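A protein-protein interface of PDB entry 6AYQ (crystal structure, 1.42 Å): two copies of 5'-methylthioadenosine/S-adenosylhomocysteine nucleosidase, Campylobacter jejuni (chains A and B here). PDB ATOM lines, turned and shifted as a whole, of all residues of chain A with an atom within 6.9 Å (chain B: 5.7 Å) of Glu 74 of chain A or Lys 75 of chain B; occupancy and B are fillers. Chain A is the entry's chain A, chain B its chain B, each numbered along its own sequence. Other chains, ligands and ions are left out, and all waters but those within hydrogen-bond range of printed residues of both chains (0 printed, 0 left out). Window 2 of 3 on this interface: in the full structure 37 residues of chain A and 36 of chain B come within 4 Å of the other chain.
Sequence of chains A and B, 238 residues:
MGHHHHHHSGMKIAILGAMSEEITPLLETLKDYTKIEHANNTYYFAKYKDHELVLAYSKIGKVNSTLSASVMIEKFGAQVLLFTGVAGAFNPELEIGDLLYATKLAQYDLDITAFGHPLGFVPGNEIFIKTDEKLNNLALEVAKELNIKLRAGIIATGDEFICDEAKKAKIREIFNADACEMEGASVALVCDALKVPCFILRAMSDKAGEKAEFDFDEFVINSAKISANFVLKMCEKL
Of the 12 printed residues of chain A, 5 touch a printed residue of chain B. Of the 11 printed residues of chain B, 6 touch a printed residue of chain A. Among the printed residues, no Asp or Glu carboxylate lies within 4 Å of a Lys or Arg side-chain nitrogen of the other chain.
Printed residues of chain B within 4 Å of Val 71 of chain A: Glu 74. Glu 74 of chain A touches just these residues of chain B: His 38 (2.6 Å), Val 71 (3.6 Å) and Lys 75 (3.8 Å). Of the printed residues of chain B, Lys 75 of chain A touches Glu 74. Ala 78 of chain A touches none of the printed residues of chain B. Printed residues of chain A within 4 Å of His 38 of chain B: Glu 74 and Leu 194. Of the printed residues of chain A, Val 71 of chain B touches Glu 74. Printed residues of chain A within 4 Å of Glu 74 of chain B: Val 71 and Lys 75. The nearest residue of chain B that does not touch Glu 74 of chain A is Glu 74 of chain B (4.2 Å).
The backbone carbonyl oxygen of Val 71 of chain A is in hydrogen-bond range of the backbone NH of Phe 76 of chain A (3.0 Å). N of Phe 76 of chain B is in hydrogen-bond range of O of Val 71 of chain B (3.2 Å).
Ser 70 of chain A touches its own counterpart, Ser 70 of chain B. Val 71 of chain A touches Glu 74 of chain B, and with the chains exchanged Glu 74 of chain A touches Val 71 of chain B. Glu 74 of chain A touches Lys 75 of chain B, and with the chains exchanged Lys 75 of chain A touches Glu 74 of chain B. 8 positions are printed for both chains.
The side-chain carboxylate of Glu 74 of chain A sits at hydrogen-bond distance from a ring nitrogen (NE2) of His 38 of chain B (2.6 Å).
Among the printed residues, pairs that only touch across the chains: Ser 70 of chain A with Ser 70 of chain B, Val 71 of chain A with Glu 74 of chain B, Glu 74 of chain A with Val 71 of chain B, Glu 74 of chain A with Lys 75 of chain B, Lys 75 of chain A with Glu 74 of chain B, Leu 194 of chain A with His 38 of chain B and Leu 194 of chain A with Ala 39 of chain B.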
ATOM      1  N   ALA A  69      17.070  10.000  20.770  1.00  0.00           N
ATOM      2  CA  ALA A  69      18.333   9.271  20.890  1.00  0.00           C
ATOM      3  C   ALA A  69      18.876   8.972  19.498  1.00  0.00           C
ATOM      4  O   ALA A  69      20.073   9.136  19.242  1.00  0.00           O
ATOM      5  CB  ALA A  69      18.161   7.995  21.698  1.00  0.00           C
ATOM      6  N   SER A  70      17.987   8.568  18.588  1.00  0.00           N
ATOM      7  CA  SER A  70      18.403   8.261  17.220  1.00  0.00           C
ATOM      8  C   SER A  70      18.919   9.511  16.506  1.00  0.00           C
ATOM      9  O   SER A  70      19.930   9.453  15.798  1.00  0.00           O
ATOM     10  CB  SER A  70      17.265   7.624  16.425  1.00  0.00           C
ATOM     11  OG  SER A  70      17.683   7.379  15.089  1.00  0.00           O
ATOM     12  N   VAL A  71      18.251  10.645  16.695  1.00  0.00           N
ATOM     13  CA  VAL A  71      18.734  11.923  16.112  1.00  0.00           C
ATOM     14  C   VAL A  71      20.113  12.313  16.647  1.00  0.00           C
ATOM     15  O   VAL A  71      21.006  12.704  15.885  1.00  0.00           O
ATOM     16  CB  VAL A  71      17.726  13.056  16.380  1.00  0.00           C
ATOM     17  CG1 VAL A  71      18.352  14.436  16.143  1.00  0.00           C
ATOM     18  CG2 VAL A  71      16.495  12.844  15.515  1.00  0.00           C
ATOM     19  N   MET A  72      20.287  12.217  17.958  1.00  0.00           N
ATOM     20  CA  MET A  72      21.535  12.620  18.596  1.00  0.00           C
ATOM     21  C   MET A  72      22.715  11.808  18.080  1.00  0.00           C
ATOM     22  O   MET A  72      23.815  12.352  17.930  1.00  0.00           O
ATOM     23  CB  MET A  72      21.417  12.531  20.108  1.00  0.00           C
ATOM     24  CG  MET A  72      20.560  13.660  20.654  1.00  0.00           C
ATOM     25  SD  MET A  72      20.066  13.424  22.354  1.00  0.00           S
ATOM     26  CE  MET A  72      20.621  14.950  23.111  1.00  0.00           C
ATOM     27  N   ILE A  73      22.475  10.533  17.783  1.00  0.00           N
ATOM     28  CA  ILE A  73      23.529   9.632  17.309  1.00  0.00           C
ATOM     29  C   ILE A  73      23.637   9.655  15.778  1.00  0.00           C
ATOM     30  O   ILE A  73      24.701   9.994  15.227  1.00  0.00           O
ATOM     31  CB  ILE A  73      23.296   8.199  17.832  1.00  0.00           C
ATOM     32  CG1 ILE A  73      23.397   8.182  19.360  1.00  0.00           C
ATOM     33  CG2 ILE A  73      24.323   7.225  17.242  1.00  0.00           C
ATOM     34  CD1 ILE A  73      22.867   6.929  20.035  1.00  0.00           C
ATOM     35  N   GLU A  74      22.552   9.319  15.088  1.00  0.00           N
ATOM     36  CA  GLU A  74      22.574   9.169  13.616  1.00  0.00           C
ATOM     37  C   GLU A  74      22.753  10.471  12.856  1.00  0.00           C
ATOM     38  O   GLU A  74      23.458  10.493  11.835  1.00  0.00           O
ATOM     39  CB  GLU A  74      21.303   8.473  13.103  1.00  0.00           C
ATOM     40  CG  GLU A  74      21.095   7.060  13.629  1.00  0.00           C
ATOM     41  CD  GLU A  74      22.078   6.053  13.065  1.00  0.00           C
ATOM     42  OE1 GLU A  74      21.655   5.224  12.242  1.00  0.00           O
ATOM     43  OE2 GLU A  74      23.257   6.072  13.465  1.00  0.00           O
ATOM     44  N   LYS A  75      22.104  11.538  13.306  1.00  0.00           N
ATOM     45  CA  LYS A  75      22.267  12.858  12.688  1.00  0.00           C
ATOM     46  C   LYS A  75      23.507  13.532  13.267  1.00  0.00           C
ATOM     47  O   LYS A  75      24.461  13.802  12.539  1.00  0.00           O
ATOM     48  CB  LYS A  75      21.005  13.721  12.878  1.00  0.00           C
ATOM     49  CG  LYS A  75      21.088  15.181  12.429  1.00  0.00           C
ATOM     50  CD  LYS A  75      21.060  15.372  10.930  1.00  0.00           C
ATOM     51  CE  LYS A  75      20.960  16.860  10.618  1.00  0.00           C
ATOM     52  NZ  LYS A  75      21.202  17.139   9.181  1.00  0.00           N
ATOM     53  N   PHE A  76      23.531  13.771  14.576  1.00  0.00           N
ATOM     54  CA  PHE A  76      24.570  14.641  15.153  1.00  0.00           C
ATOM     55  C   PHE A  76      25.860  13.946  15.600  1.00  0.00           C
ATOM     56  O   PHE A  76      26.795  14.623  16.026  1.00  0.00           O
ATOM     57  CB  PHE A  76      23.973  15.519  16.252  1.00  0.00           C
ATOM     58  CG  PHE A  76      22.897  16.452  15.755  1.00  0.00           C
ATOM     59  CD1 PHE A  76      23.162  17.356  14.721  1.00  0.00           C
ATOM     60  CD2 PHE A  76      21.618  16.418  16.284  1.00  0.00           C
ATOM     61  CE1 PHE A  76      22.188  18.211  14.251  1.00  0.00           C
ATOM     62  CE2 PHE A  76      20.639  17.281  15.814  1.00  0.00           C
ATOM     63  CZ  PHE A  76      20.929  18.176  14.793  1.00  0.00           C
ATOM     64  N   GLY A  77      25.924  12.624  15.486  1.00  0.00           N
ATOM     65  CA  GLY A  77      27.167  11.879  15.742  1.00  0.00           C
ATOM     66  C   GLY A  77      27.618  11.777  17.184  1.00  0.00           C
ATOM     67  O   GLY A  77      28.806  11.591  17.462  1.00  0.00           O
ATOM     68  N   ALA A  78      26.691  11.855  18.137  1.00  0.00           N
ATOM     69  CA  ALA A  78      27.057  11.632  19.526  1.00  0.00           C
ATOM     70  C   ALA A  78      27.686  10.238  19.701  1.00  0.00           C
ATOM     71  O   ALA A  78      27.253   9.259  19.070  1.00  0.00           O
ATOM     72  CB  ALA A  78      25.849  11.784  20.433  1.00  0.00           C
ATOM     73  N   VAL A 190      18.066   2.067  21.674  1.00  0.00           N
ATOM     74  CA  VAL A 190      18.670   2.817  20.573  1.00  0.00           C
ATOM     75  C   VAL A 190      20.190   2.825  20.697  1.00  0.00           C
ATOM     76  O   VAL A 190      20.909   2.553  19.720  1.00  0.00           O
ATOM     77  CB  VAL A 190      18.131   4.260  20.493  1.00  0.00           C
ATOM     78  CG1 VAL A 190      18.892   5.076  19.458  1.00  0.00           C
ATOM     79  CG2 VAL A 190      16.653   4.270  20.147  1.00  0.00           C
ATOM     80  N   LEU A 194      22.952   1.095  18.122  1.00  0.00           N
ATOM     81  CA  LEU A 194      23.892   1.955  17.399  1.00  0.00           C
ATOM     82  C   LEU A 194      25.305   1.931  17.980  1.00  0.00           C
ATOM     83  O   LEU A 194      26.147   2.747  17.582  1.00  0.00           O
ATOM     84  CB  LEU A 194      23.356   3.382  17.368  1.00  0.00           C
ATOM     85  CG  LEU A 194      22.004   3.544  16.673  1.00  0.00           C
ATOM     86  CD1 LEU A 194      21.525   4.973  16.751  1.00  0.00           C
ATOM     87  CD2 LEU A 194      22.050   3.099  15.219  1.00  0.00           C
ATOM     88  N   ILE B  36      22.782  -3.848   3.940  1.00  0.00           N
ATOM     89  CA  ILE B  36      23.706  -3.306   4.946  1.00  0.00           C
ATOM     90  C   ILE B  36      23.178  -3.656   6.338  1.00  0.00           C
ATOM     91  O   ILE B  36      21.979  -3.505   6.604  1.00  0.00           O
ATOM     92  CB  ILE B  36      23.864  -1.776   4.810  1.00  0.00           C
ATOM     93  CG1 ILE B  36      24.520  -1.438   3.463  1.00  0.00           C
ATOM     94  CG2 ILE B  36      24.689  -1.199   5.964  1.00  0.00           C
ATOM     95  CD1 ILE B  36      24.574   0.039   3.125  1.00  0.00           C
ATOM     96  N   HIS B  38      22.918  -2.665  10.050  1.00  0.00           N
ATOM     97  CA  HIS B  38      22.989  -1.424  10.839  1.00  0.00           C
ATOM     98  C   HIS B  38      21.862  -1.371  11.863  1.00  0.00           C
ATOM     99  O   HIS B  38      20.768  -1.866  11.596  1.00  0.00           O
ATOM    100  CB  HIS B  38      22.891  -0.208   9.928  1.00  0.00           C
ATOM    101  CG  HIS B  38      23.114   1.092  10.636  1.00  0.00           C
ATOM    102  ND1 HIS B  38      24.344   1.476  11.121  1.00  0.00           N
ATOM    103  CD2 HIS B  38      22.255   2.093  10.946  1.00  0.00           C
ATOM    104  CE1 HIS B  38      24.233   2.661  11.696  1.00  0.00           C
ATOM    105  NE2 HIS B  38      22.976   3.057  11.605  1.00  0.00           N
ATOM    106  N   ALA B  39      22.140  -0.784  13.028  1.00  0.00           N
ATOM    107  CA  ALA B  39      21.128  -0.611  14.075  1.00  0.00           C
ATOM    108  C   ALA B  39      20.450  -1.932  14.465  1.00  0.00           C
ATOM    109  O   ALA B  39      19.229  -1.987  14.655  1.00  0.00           O
ATOM    110  CB  ALA B  39      20.107   0.433  13.641  1.00  0.00           C
ATOM    111  N   SER B  70      13.588   6.359  11.638  1.00  0.00           N
ATOM    112  CA  SER B  70      14.616   7.377  11.887  1.00  0.00           C
ATOM    113  C   SER B  70      15.908   7.052  11.141  1.00  0.00           C
ATOM    114  O   SER B  70      16.552   7.942  10.564  1.00  0.00           O
ATOM    115  CB  SER B  70      14.912   7.494  13.391  1.00  0.00           C
ATOM    116  OG  SER B  70      13.792   7.955  14.118  1.00  0.00           O
ATOM    117  N   VAL B  71      16.302   5.780  11.169  1.00  0.00           N
ATOM    118  CA  VAL B  71      17.512   5.326  10.467  1.00  0.00           C
ATOM    119  C   VAL B  71      17.356   5.507   8.959  1.00  0.00           C
ATOM    120  O   VAL B  71      18.263   6.001   8.293  1.00  0.00           O
ATOM    121  CB  VAL B  71      17.838   3.859  10.816  1.00  0.00           C
ATOM    122  CG1 VAL B  71      18.889   3.271   9.875  1.00  0.00           C
ATOM    123  CG2 VAL B  71      18.321   3.777  12.259  1.00  0.00           C
ATOM    124  N   MET B  72      16.206   5.127   8.419  1.00  0.00           N
ATOM    125  CA  MET B  72      16.005   5.176   6.972  1.00  0.00           C
ATOM    126  C   MET B  72      16.064   6.596   6.442  1.00  0.00           C
ATOM    127  O   MET B  72      16.536   6.815   5.328  1.00  0.00           O
ATOM    128  CB  MET B  72      14.675   4.510   6.602  1.00  0.00           C
ATOM    129  CG  MET B  72      14.697   3.009   6.803  1.00  0.00           C
ATOM    130  SD  MET B  72      13.066   2.239   6.775  1.00  0.00           S
ATOM    131  CE  MET B  72      13.167   1.271   5.269  1.00  0.00           C
ATOM    132  N   ILE B  73      15.591   7.550   7.240  1.00  0.00           N
ATOM    133  CA  ILE B  73      15.586   8.964   6.872  1.00  0.00           C
ATOM    134  C   ILE B  73      16.945   9.600   7.203  1.00  0.00           C
ATOM    135  O   ILE B  73      17.583  10.166   6.315  1.00  0.00           O
ATOM    136  CB  ILE B  73      14.429   9.722   7.563  1.00  0.00           C
ATOM    137  CG1 ILE B  73      13.082   9.167   7.085  1.00  0.00           C
ATOM    138  CG2 ILE B  73      14.505  11.216   7.274  1.00  0.00           C
ATOM    139  CD1 ILE B  73      11.896   9.621   7.912  1.00  0.00           C
ATOM    140  N   GLU B  74      17.382   9.514   8.460  1.00  0.00           N
ATOM    141  CA  GLU B  74      18.584  10.244   8.909  1.00  0.00           C
ATOM    142  C   GLU B  74      19.889   9.671   8.357  1.00  0.00           C
ATOM    143  O   GLU B  74      20.820  10.446   8.074  1.00  0.00           O
ATOM    144  CB  GLU B  74      18.670  10.310  10.441  1.00  0.00           C
ATOM    145  CG  GLU B  74      17.522  11.023  11.150  1.00  0.00           C
ATOM    146  CD  GLU B  74      17.543  12.535  10.994  1.00  0.00           C
ATOM    147  OE1 GLU B  74      17.593  13.241  12.016  1.00  0.00           O
ATOM    148  OE2 GLU B  74      17.493  13.027   9.850  1.00  0.00           O
ATOM    149  N   LYS B  75      19.980   8.346   8.220  1.00  0.00           N
ATOM    150  CA  LYS B  75      21.182   7.702   7.700  1.00  0.00           C
ATOM    151  C   LYS B  75      21.098   7.456   6.202  1.00  0.00           C
ATOM    152  O   LYS B  75      22.021   7.816   5.471  1.00  0.00           O
ATOM    153  CB  LYS B  75      21.485   6.389   8.422  1.00  0.00           C
ATOM    154  CG  LYS B  75      22.789   5.745   7.961  1.00  0.00           C
ATOM    155  CD  LYS B  75      23.154   4.547   8.805  1.00  0.00           C
ATOM    156  CE  LYS B  75      24.429   3.877   8.316  1.00  0.00           C
ATOM    157  NZ  LYS B  75      25.639   4.713   8.551  1.00  0.00           N
ATOM    158  N   PHE B  76      20.019   6.826   5.742  1.00  0.00           N
ATOM    159  CA  PHE B  76      19.928   6.404   4.341  1.00  0.00           C
ATOM    160  C   PHE B  76      19.176   7.386   3.428  1.00  0.00           C
ATOM    161  O   PHE B  76      18.962   7.084   2.255  1.00  0.00           O
ATOM    162  CB  PHE B  76      19.356   4.983   4.260  1.00  0.00           C
ATOM    163  CG  PHE B  76      20.178   3.961   5.008  1.00  0.00           C
ATOM    164  CD1 PHE B  76      21.527   3.764   4.696  1.00  0.00           C
ATOM    165  CD2 PHE B  76      19.613   3.175   6.020  1.00  0.00           C
ATOM    166  CE1 PHE B  76      22.289   2.820   5.378  1.00  0.00           C
ATOM    167  CE2 PHE B  76      20.372   2.228   6.702  1.00  0.00           C
ATOM    168  CZ  PHE B  76      21.712   2.045   6.380  1.00  0.00           C
ATOM    169  N   GLY B  77      18.791   8.550   3.951  1.00  0.00           N
ATOM    170  CA  GLY B  77      18.284   9.667   3.138  1.00  0.00           C
ATOM    171  C   GLY B  77      16.941   9.492   2.452  1.00  0.00           C
ATOM    172  O   GLY B  77      16.678  10.105   1.407  1.00  0.00           O
